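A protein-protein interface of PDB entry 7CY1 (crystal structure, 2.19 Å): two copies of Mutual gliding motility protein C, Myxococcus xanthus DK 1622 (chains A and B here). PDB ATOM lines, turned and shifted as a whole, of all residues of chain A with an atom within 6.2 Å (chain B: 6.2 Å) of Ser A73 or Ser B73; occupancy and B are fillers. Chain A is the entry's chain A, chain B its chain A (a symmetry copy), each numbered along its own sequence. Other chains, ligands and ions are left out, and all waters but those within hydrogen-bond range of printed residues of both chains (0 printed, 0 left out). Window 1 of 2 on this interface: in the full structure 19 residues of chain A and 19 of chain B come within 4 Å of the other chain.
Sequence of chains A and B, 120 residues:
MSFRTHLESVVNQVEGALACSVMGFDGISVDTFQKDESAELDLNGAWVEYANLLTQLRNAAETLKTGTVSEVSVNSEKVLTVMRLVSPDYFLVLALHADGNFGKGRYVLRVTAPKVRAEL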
ATOM      1  N   LEU A  57     -34.450 -13.407   8.757  1.00  0.00           N
ATOM      2  CA  LEU A  57     -34.279 -12.101   9.440  1.00  0.00           C
ATOM      3  C   LEU A  57     -33.851 -12.380  10.876  1.00  0.00           C
ATOM      4  O   LEU A  57     -32.799 -11.875  11.281  1.00  0.00           O
ATOM      5  CB  LEU A  57     -35.576 -11.290   9.380  1.00  0.00           C
ATOM      6  CG  LEU A  57     -35.883 -10.735   7.995  1.00  0.00           C
ATOM      7  CD1 LEU A  57     -37.235 -10.053   7.946  1.00  0.00           C
ATOM      8  CD2 LEU A  57     -34.800  -9.766   7.564  1.00  0.00           C
ATOM      9  N   ALA A  60     -30.175 -13.750  11.192  1.00  0.00           N
ATOM     10  CA  ALA A  60     -29.143 -12.716  10.951  1.00  0.00           C
ATOM     11  C   ALA A  60     -29.152 -11.671  12.078  1.00  0.00           C
ATOM     12  O   ALA A  60     -28.080 -11.134  12.405  1.00  0.00           O
ATOM     13  CB  ALA A  60     -29.387 -12.070   9.610  1.00  0.00           C
ATOM     14  N   GLU A  71     -26.092  -2.700  12.667  1.00  0.00           N
ATOM     15  CA  GLU A  71     -27.111  -2.690  11.584  1.00  0.00           C
ATOM     16  C   GLU A  71     -26.948  -3.955  10.720  1.00  0.00           C
ATOM     17  O   GLU A  71     -25.805  -4.284  10.332  1.00  0.00           O
ATOM     18  CB  GLU A  71     -26.923  -1.370  10.828  1.00  0.00           C
ATOM     19  CG  GLU A  71     -27.902  -1.079   9.709  1.00  0.00           C
ATOM     20  CD  GLU A  71     -27.434   0.112   8.870  1.00  0.00           C
ATOM     21  OE1 GLU A  71     -26.399  -0.015   8.183  1.00  0.00           O
ATOM     22  OE2 GLU A  71     -28.067   1.189   8.939  1.00  0.00           O
ATOM     23  N   VAL A  72     -28.043  -4.673  10.450  1.00  0.00           N
ATOM     24  CA  VAL A  72     -28.050  -5.889   9.582  1.00  0.00           C
ATOM     25  C   VAL A  72     -29.145  -5.732   8.525  1.00  0.00           C
ATOM     26  O   VAL A  72     -30.191  -5.150   8.822  1.00  0.00           O
ATOM     27  CB  VAL A  72     -28.227  -7.165  10.418  1.00  0.00           C
ATOM     28  CG1 VAL A  72     -28.330  -8.424   9.563  1.00  0.00           C
ATOM     29  CG2 VAL A  72     -27.086  -7.281  11.413  1.00  0.00           C
ATOM     30  N   SER A  73     -28.885  -6.208   7.313  1.00  0.00           N
ATOM     31  CA  SER A  73     -29.847  -6.144   6.187  1.00  0.00           C
ATOM     32  C   SER A  73     -29.910  -7.532   5.542  1.00  0.00           C
ATOM     33  O   SER A  73     -28.869  -8.164   5.371  1.00  0.00           O
ATOM     34  CB  SER A  73     -29.496  -4.997   5.254  1.00  0.00           C
ATOM     35  OG  SER A  73     -29.974  -5.227   3.935  1.00  0.00           O
ATOM     36  N   VAL A  74     -31.115  -8.071   5.381  1.00  0.00           N
ATOM     37  CA  VAL A  74     -31.342  -9.376   4.709  1.00  0.00           C
ATOM     38  C   VAL A  74     -32.357  -9.101   3.601  1.00  0.00           C
ATOM     39  O   VAL A  74     -33.529  -8.702   3.922  1.00  0.00           O
ATOM     40  CB  VAL A  74     -31.811 -10.479   5.671  1.00  0.00           C
ATOM     41  CG1 VAL A  74     -32.130 -11.748   4.914  1.00  0.00           C
ATOM     42  CG2 VAL A  74     -30.807 -10.779   6.773  1.00  0.00           C
ATOM     43  N   ASN A  75     -31.899  -9.208   2.356  1.00  0.00           N
ATOM     44  CA  ASN A  75     -32.600  -8.643   1.184  1.00  0.00           C
ATOM     45  C   ASN A  75     -32.879  -9.749   0.180  1.00  0.00           C
ATOM     46  O   ASN A  75     -32.065 -10.690   0.056  1.00  0.00           O
ATOM     47  CB  ASN A  75     -31.798  -7.574   0.449  1.00  0.00           C
ATOM     48  CG  ASN A  75     -31.552  -6.344   1.282  1.00  0.00           C
ATOM     49  OD1 ASN A  75     -32.174  -6.168   2.324  1.00  0.00           O
ATOM     50  ND2 ASN A  75     -30.637  -5.509   0.826  1.00  0.00           N
ATOM     51  N   LEU A  80     -36.172  -5.253   0.654  1.00  0.00           N
ATOM     52  CA  LEU A  80     -34.972  -4.826   1.401  1.00  0.00           C
ATOM     53  C   LEU A  80     -35.413  -4.714   2.860  1.00  0.00           C
ATOM     54  O   LEU A  80     -36.588  -4.355   3.078  1.00  0.00           O
ATOM     55  CB  LEU A  80     -34.453  -3.493   0.854  1.00  0.00           C
ATOM     56  CG  LEU A  80     -34.425  -3.347  -0.664  1.00  0.00           C
ATOM     57  CD1 LEU A  80     -33.926  -1.962  -1.065  1.00  0.00           C
ATOM     58  CD2 LEU A  80     -33.570  -4.432  -1.312  1.00  0.00           C
ATOM     59  N   THR A  81     -34.560  -5.134   3.795  1.00  0.00           N
ATOM     60  CA  THR A  81     -34.782  -4.973   5.252  1.00  0.00           C
ATOM     61  C   THR A  81     -33.576  -4.254   5.853  1.00  0.00           C
ATOM     62  O   THR A  81     -32.470  -4.363   5.293  1.00  0.00           O
ATOM     63  CB  THR A  81     -35.084  -6.297   5.947  1.00  0.00           C
ATOM     64  OG1 THR A  81     -33.942  -7.142   5.889  1.00  0.00           O
ATOM     65  CG2 THR A  81     -36.265  -7.011   5.331  1.00  0.00           C
ATOM     66  N   VAL A  82     -33.817  -3.492   6.909  1.00  0.00           N
ATOM     67  CA  VAL A  82     -32.762  -2.929   7.787  1.00  0.00           C
ATOM     68  C   VAL A  82     -33.159  -3.294   9.211  1.00  0.00           C
ATOM     69  O   VAL A  82     -34.341  -3.173   9.539  1.00  0.00           O
ATOM     70  CB  VAL A  82     -32.652  -1.403   7.663  1.00  0.00           C
ATOM     71  CG1 VAL A  82     -31.328  -0.928   8.231  1.00  0.00           C
ATOM     72  CG2 VAL A  82     -32.852  -0.927   6.242  1.00  0.00           C
ATOM     73  N   MET A  83     -32.216  -3.749  10.019  1.00  0.00           N
ATOM     74  CA  MET A  83     -32.513  -4.128  11.405  1.00  0.00           C
ATOM     75  C   MET A  83     -31.482  -3.478  12.320  1.00  0.00           C
ATOM     76  O   MET A  83     -30.301  -3.411  11.923  1.00  0.00           O
ATOM     77  CB  MET A  83     -32.497  -5.651  11.542  1.00  0.00           C
ATOM     78  CG  MET A  83     -33.434  -6.330  10.568  1.00  0.00           C
ATOM     79  SD  MET A  83     -33.437  -8.118  10.751  1.00  0.00           S
ATOM     80  CE  MET A  83     -32.008  -8.517   9.744  1.00  0.00           C
ATOM     81  N   PHE A 102     -33.658   2.983  -0.024  1.00  0.00           N
ATOM     82  CA  PHE A 102     -32.892   2.156   0.951  1.00  0.00           C
ATOM     83  C   PHE A 102     -32.028   3.053   1.853  1.00  0.00           C
ATOM     84  O   PHE A 102     -31.972   2.832   3.092  1.00  0.00           O
ATOM     85  CB  PHE A 102     -32.080   1.080   0.220  1.00  0.00           C
ATOM     86  CG  PHE A 102     -31.464   0.033   1.122  1.00  0.00           C
ATOM     87  CD1 PHE A 102     -32.250  -0.730   1.971  1.00  0.00           C
ATOM     88  CD2 PHE A 102     -30.097  -0.194   1.128  1.00  0.00           C
ATOM     89  CE1 PHE A 102     -31.687  -1.694   2.797  1.00  0.00           C
ATOM     90  CE2 PHE A 102     -29.537  -1.157   1.955  1.00  0.00           C
ATOM     91  CZ  PHE A 102     -30.332  -1.902   2.793  1.00  0.00           C
ATOM     92  N   LEU B  57     -20.147 -12.078  10.088  1.00  0.00           N
ATOM     93  CA  LEU B  57     -20.364 -12.097   8.621  1.00  0.00           C
ATOM     94  C   LEU B  57     -20.731 -13.523   8.224  1.00  0.00           C
ATOM     95  O   LEU B  57     -21.795 -13.707   7.624  1.00  0.00           O
ATOM     96  CB  LEU B  57     -19.115 -11.605   7.886  1.00  0.00           C
ATOM     97  CG  LEU B  57     -18.882 -10.106   8.018  1.00  0.00           C
ATOM     98  CD1 LEU B  57     -17.570  -9.679   7.391  1.00  0.00           C
ATOM     99  CD2 LEU B  57     -20.028  -9.338   7.390  1.00  0.00           C
ATOM    100  N   ALA B  60     -24.318 -14.623   9.414  1.00  0.00           N
ATOM    101  CA  ALA B  60     -25.410 -13.990   8.639  1.00  0.00           C
ATOM    102  C   ALA B  60     -25.419 -14.514   7.194  1.00  0.00           C
ATOM    103  O   ALA B  60     -26.507 -14.615   6.602  1.00  0.00           O
ATOM    104  CB  ALA B  60     -25.243 -12.492   8.673  1.00  0.00           C
ATOM    105  N   GLU B  71     -28.928 -11.103  -0.945  1.00  0.00           N
ATOM    106  CA  GLU B  71     -27.946 -10.082  -0.490  1.00  0.00           C
ATOM    107  C   GLU B  71     -28.070  -9.902   1.035  1.00  0.00           C
ATOM    108  O   GLU B  71     -29.206  -9.767   1.542  1.00  0.00           O
ATOM    109  CB  GLU B  71     -28.227  -8.819  -1.310  1.00  0.00           C
ATOM    110  CG  GLU B  71     -27.302  -7.641  -1.086  1.00  0.00           C
ATOM    111  CD  GLU B  71     -27.858  -6.376  -1.745  1.00  0.00           C
ATOM    112  OE1 GLU B  71     -28.908  -5.878  -1.284  1.00  0.00           O
ATOM    113  OE2 GLU B  71     -27.281  -5.912  -2.753  1.00  0.00           O
ATOM    114  N   VAL B  72     -26.948  -9.932   1.762  1.00  0.00           N
ATOM    115  CA  VAL B  72     -26.904  -9.716   3.239  1.00  0.00           C
ATOM    116  C   VAL B  72     -25.854  -8.647   3.549  1.00  0.00           C
ATOM    117  O   VAL B  72     -24.831  -8.590   2.861  1.00  0.00           O
ATOM    118  CB  VAL B  72     -26.634 -11.031   3.984  1.00  0.00           C
ATOM    119  CG1 VAL B  72     -26.493 -10.842   5.490  1.00  0.00           C
ATOM    120  CG2 VAL B  72     -27.734 -12.028   3.667  1.00  0.00           C
ATOM    121  N   SER B  73     -26.127  -7.802   4.535  1.00  0.00           N
ATOM    122  CA  SER B  73     -25.207  -6.721   4.964  1.00  0.00           C
ATOM    123  C   SER B  73     -25.091  -6.779   6.490  1.00  0.00           C
ATOM    124  O   SER B  73     -26.102  -6.971   7.163  1.00  0.00           O
ATOM    125  CB  SER B  73     -25.647  -5.388   4.383  1.00  0.00           C
ATOM    126  OG  SER B  73     -25.201  -4.297   5.178  1.00  0.00           O
ATOM    127  N   VAL B  74     -23.865  -6.819   7.004  1.00  0.00           N
ATOM    128  CA  VAL B  74     -23.592  -6.806   8.464  1.00  0.00           C
ATOM    129  C   VAL B  74     -22.628  -5.643   8.695  1.00  0.00           C
ATOM    130  O   VAL B  74     -21.470  -5.684   8.156  1.00  0.00           O
ATOM    131  CB  VAL B  74     -23.035  -8.139   8.987  1.00  0.00           C
ATOM    132  CG1 VAL B  74     -22.674  -8.028  10.451  1.00  0.00           C
ATOM    133  CG2 VAL B  74     -23.985  -9.307   8.781  1.00  0.00           C
ATOM    134  N   ASN B  75     -23.121  -4.611   9.375  1.00  0.00           N
ATOM    135  CA  ASN B  75     -22.488  -3.274   9.388  1.00  0.00           C
ATOM    136  C   ASN B  75     -22.184  -2.873  10.822  1.00  0.00           C
ATOM    137  O   ASN B  75     -22.951  -3.235  11.741  1.00  0.00           O
ATOM    138  CB  ASN B  75     -23.368  -2.175   8.801  1.00  0.00           C
ATOM    139  CG  ASN B  75     -23.653  -2.367   7.335  1.00  0.00           C
ATOM    140  OD1 ASN B  75     -23.007  -3.179   6.681  1.00  0.00           O
ATOM    141  ND2 ASN B  75     -24.624  -1.628   6.832  1.00  0.00           N
ATOM    142  N   LEU B  80     -19.118  -1.067   6.505  1.00  0.00           N
ATOM    143  CA  LEU B  80     -20.315  -1.600   5.823  1.00  0.00           C
ATOM    144  C   LEU B  80     -19.834  -2.821   5.040  1.00  0.00           C
ATOM    145  O   LEU B  80     -18.673  -2.789   4.583  1.00  0.00           O
ATOM    146  CB  LEU B  80     -20.921  -0.533   4.906  1.00  0.00           C
ATOM    147  CG  LEU B  80     -21.005   0.881   5.473  1.00  0.00           C
ATOM    148  CD1 LEU B  80     -21.589   1.843   4.443  1.00  0.00           C
ATOM    149  CD2 LEU B  80     -21.822   0.915   6.761  1.00  0.00           C
ATOM    150  N   THR B  81     -20.633  -3.889   5.012  1.00  0.00           N
ATOM    151  CA  THR B  81     -20.373  -5.097   4.194  1.00  0.00           C
ATOM    152  C   THR B  81     -21.595  -5.366   3.318  1.00  0.00           C
ATOM    153  O   THR B  81     -22.710  -4.977   3.707  1.00  0.00           O
ATOM    154  CB  THR B  81     -19.979  -6.302   5.041  1.00  0.00           C
ATOM    155  OG1 THR B  81     -21.076  -6.698   5.855  1.00  0.00           O
ATOM    156  CG2 THR B  81     -18.783  -6.020   5.920  1.00  0.00           C
ATOM    157  N   VAL B  82     -21.361  -5.943   2.149  1.00  0.00           N
ATOM    158  CA  VAL B  82     -22.415  -6.522   1.282  1.00  0.00           C
ATOM    159  C   VAL B  82     -21.954  -7.932   0.940  1.00  0.00           C
ATOM    160  O   VAL B  82     -20.770  -8.106   0.644  1.00  0.00           O
ATOM    161  CB  VAL B  82     -22.609  -5.721  -0.014  1.00  0.00           C
ATOM    162  CG1 VAL B  82     -23.938  -6.078  -0.653  1.00  0.00           C
ATOM    163  CG2 VAL B  82     -22.481  -4.231   0.208  1.00  0.00           C
ATOM    164  N   MET B  83     -22.845  -8.907   1.003  1.00  0.00           N
ATOM    165  CA  MET B  83     -22.484 -10.296   0.695  1.00  0.00           C
ATOM    166  C   MET B  83     -23.518 -10.866  -0.268  1.00  0.00           C
ATOM    167  O   MET B  83     -24.714 -10.545  -0.107  1.00  0.00           O
ATOM    168  CB  MET B  83     -22.415 -11.114   1.986  1.00  0.00           C
ATOM    169  CG  MET B  83     -21.476 -10.509   3.005  1.00  0.00           C
ATOM    170  SD  MET B  83     -21.373 -11.487   4.509  1.00  0.00           S
ATOM    171  CE  MET B  83     -22.811 -10.851   5.371  1.00  0.00           C
ATOM    172  N   PHE B 102     -22.084   3.161  -0.417  1.00  0.00           N
ATOM    173  CA  PHE B 102     -22.773   1.879  -0.106  1.00  0.00           C
ATOM    174  C   PHE B 102     -23.654   1.441  -1.289  1.00  0.00           C
ATOM    175  O   PHE B 102     -23.658   0.236  -1.658  1.00  0.00           O
ATOM    176  CB  PHE B 102     -23.550   1.992   1.211  1.00  0.00           C
ATOM    177  CG  PHE B 102     -24.081   0.681   1.747  1.00  0.00           C
ATOM    178  CD1 PHE B 102     -23.229  -0.380   2.011  1.00  0.00           C
ATOM    179  CD2 PHE B 102     -25.434   0.501   1.989  1.00  0.00           C
ATOM    180  CE1 PHE B 102     -23.714  -1.583   2.506  1.00  0.00           C
ATOM    181  CE2 PHE B 102     -25.915  -0.702   2.485  1.00  0.00           C
ATOM    182  CZ  PHE B 102     -25.055  -1.746   2.737  1.00  0.00           C
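OD1 of Asn A75 sits at hydrogen-bond distance from OG of Ser A73, 2.9 Å away.
The side-chain hydroxyl (OG) of Ser A73 lies within hydrogen-bond range of the backbone carbonyl oxygen (O) of Thr A81 (3.0 Å).
The side-chain amide oxygen (OD1) of Asn A75 sits at hydrogen-bond distance from the backbone NH (N) of Thr A81 (3.0 Å).
The side-chain hydroxyl (OG) of Ser B73 is in hydrogen-bond range of the backbone carbonyl oxygen (O) of Thr B81 (3.0 Å).
The backbone carbonyl oxygen (O) of Val B74 is in hydrogen-bond range of the side-chain hydroxyl (OG1) of Thr B81 (2.5 Å).
The backbone NH (N) of Thr B81 is in hydrogen-bond range of the side-chain amide oxygen (OD1) of Asn B75.
OE1 of Glu A71 lies within hydrogen-bond range of ND2 of Asn B75 (2.8 Å).
The backbone NH of Ser A73 lies within hydrogen-bond range of the backbone carbonyl oxygen of Ser B73, 2.9 Å away.
The side-chain amide nitrogen of Asn A75 is in hydrogen-bond range of the side-chain carboxylate of Glu B71, 2.8 Å away.
Glu A71 touches Val B74, and with the chains exchanged Val A74 touches Glu B71.
Glu A71 touches Asn B75, and with the chains exchanged Asn A75 touches Glu B71.
Val A72 touches Ser B73, and with the chains exchanged Ser A73 touches Val B72.
Ser A73 touches its own counterpart, Ser B73.
Glu A71 touches Val B74 (O to C, 3.8 Å).
Val A72 touches Ser B73.
Val B72 touches Ser A73 (CA to O, 3.3 Å).
Glu B71 touches Val A74 (O to C, 3.8 Å).
CE2 of Phe B102 touches CE2 of Phe A102, 3.7 Å away.
Ala A60 touches none of the printed residues of chain B.
Printed residues of chain B within 4 Å of Glu A71: Val B74 and Asn B75.
Ser A73 touches two residues of chain B.
Met A83 touches none of the printed residues of chain B.
Ser B73 touches two residues of chain A.
Printed residues of chain A within 4 Å of Val B74: Glu A71.
The nearest residue of chain B that does not touch Ser A73 is Glu B71 (4.2 Å).
The nearest residue of chain A that does not touch Ser B73 is Glu A71 (4.2 Å).
The nearest printed residue of chain B that does not touch Val A74 is Val B72 (4.5 Å).
Printed residues of chain B that touch a printed residue of chain A: Glu B71, Val B72, Ser B73, Val B74, Asn B75 and Phe B102.
Hydrophobic or aromatic side chains of chain B within 4 Å of the printed part of chain A: Val B72 and Phe B102.
Hydrophobic or aromatic side chains of chain A that line the printed part of chain B: Val A72 and Phe A102.
Along chain A the printed residues that touch a printed residue of chain B span positions 71 to 102.
Among the printed residues, no Asp or Glu carboxylate lies within 4 Å of a Lys or Arg side-chain nitrogen of the other chain.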
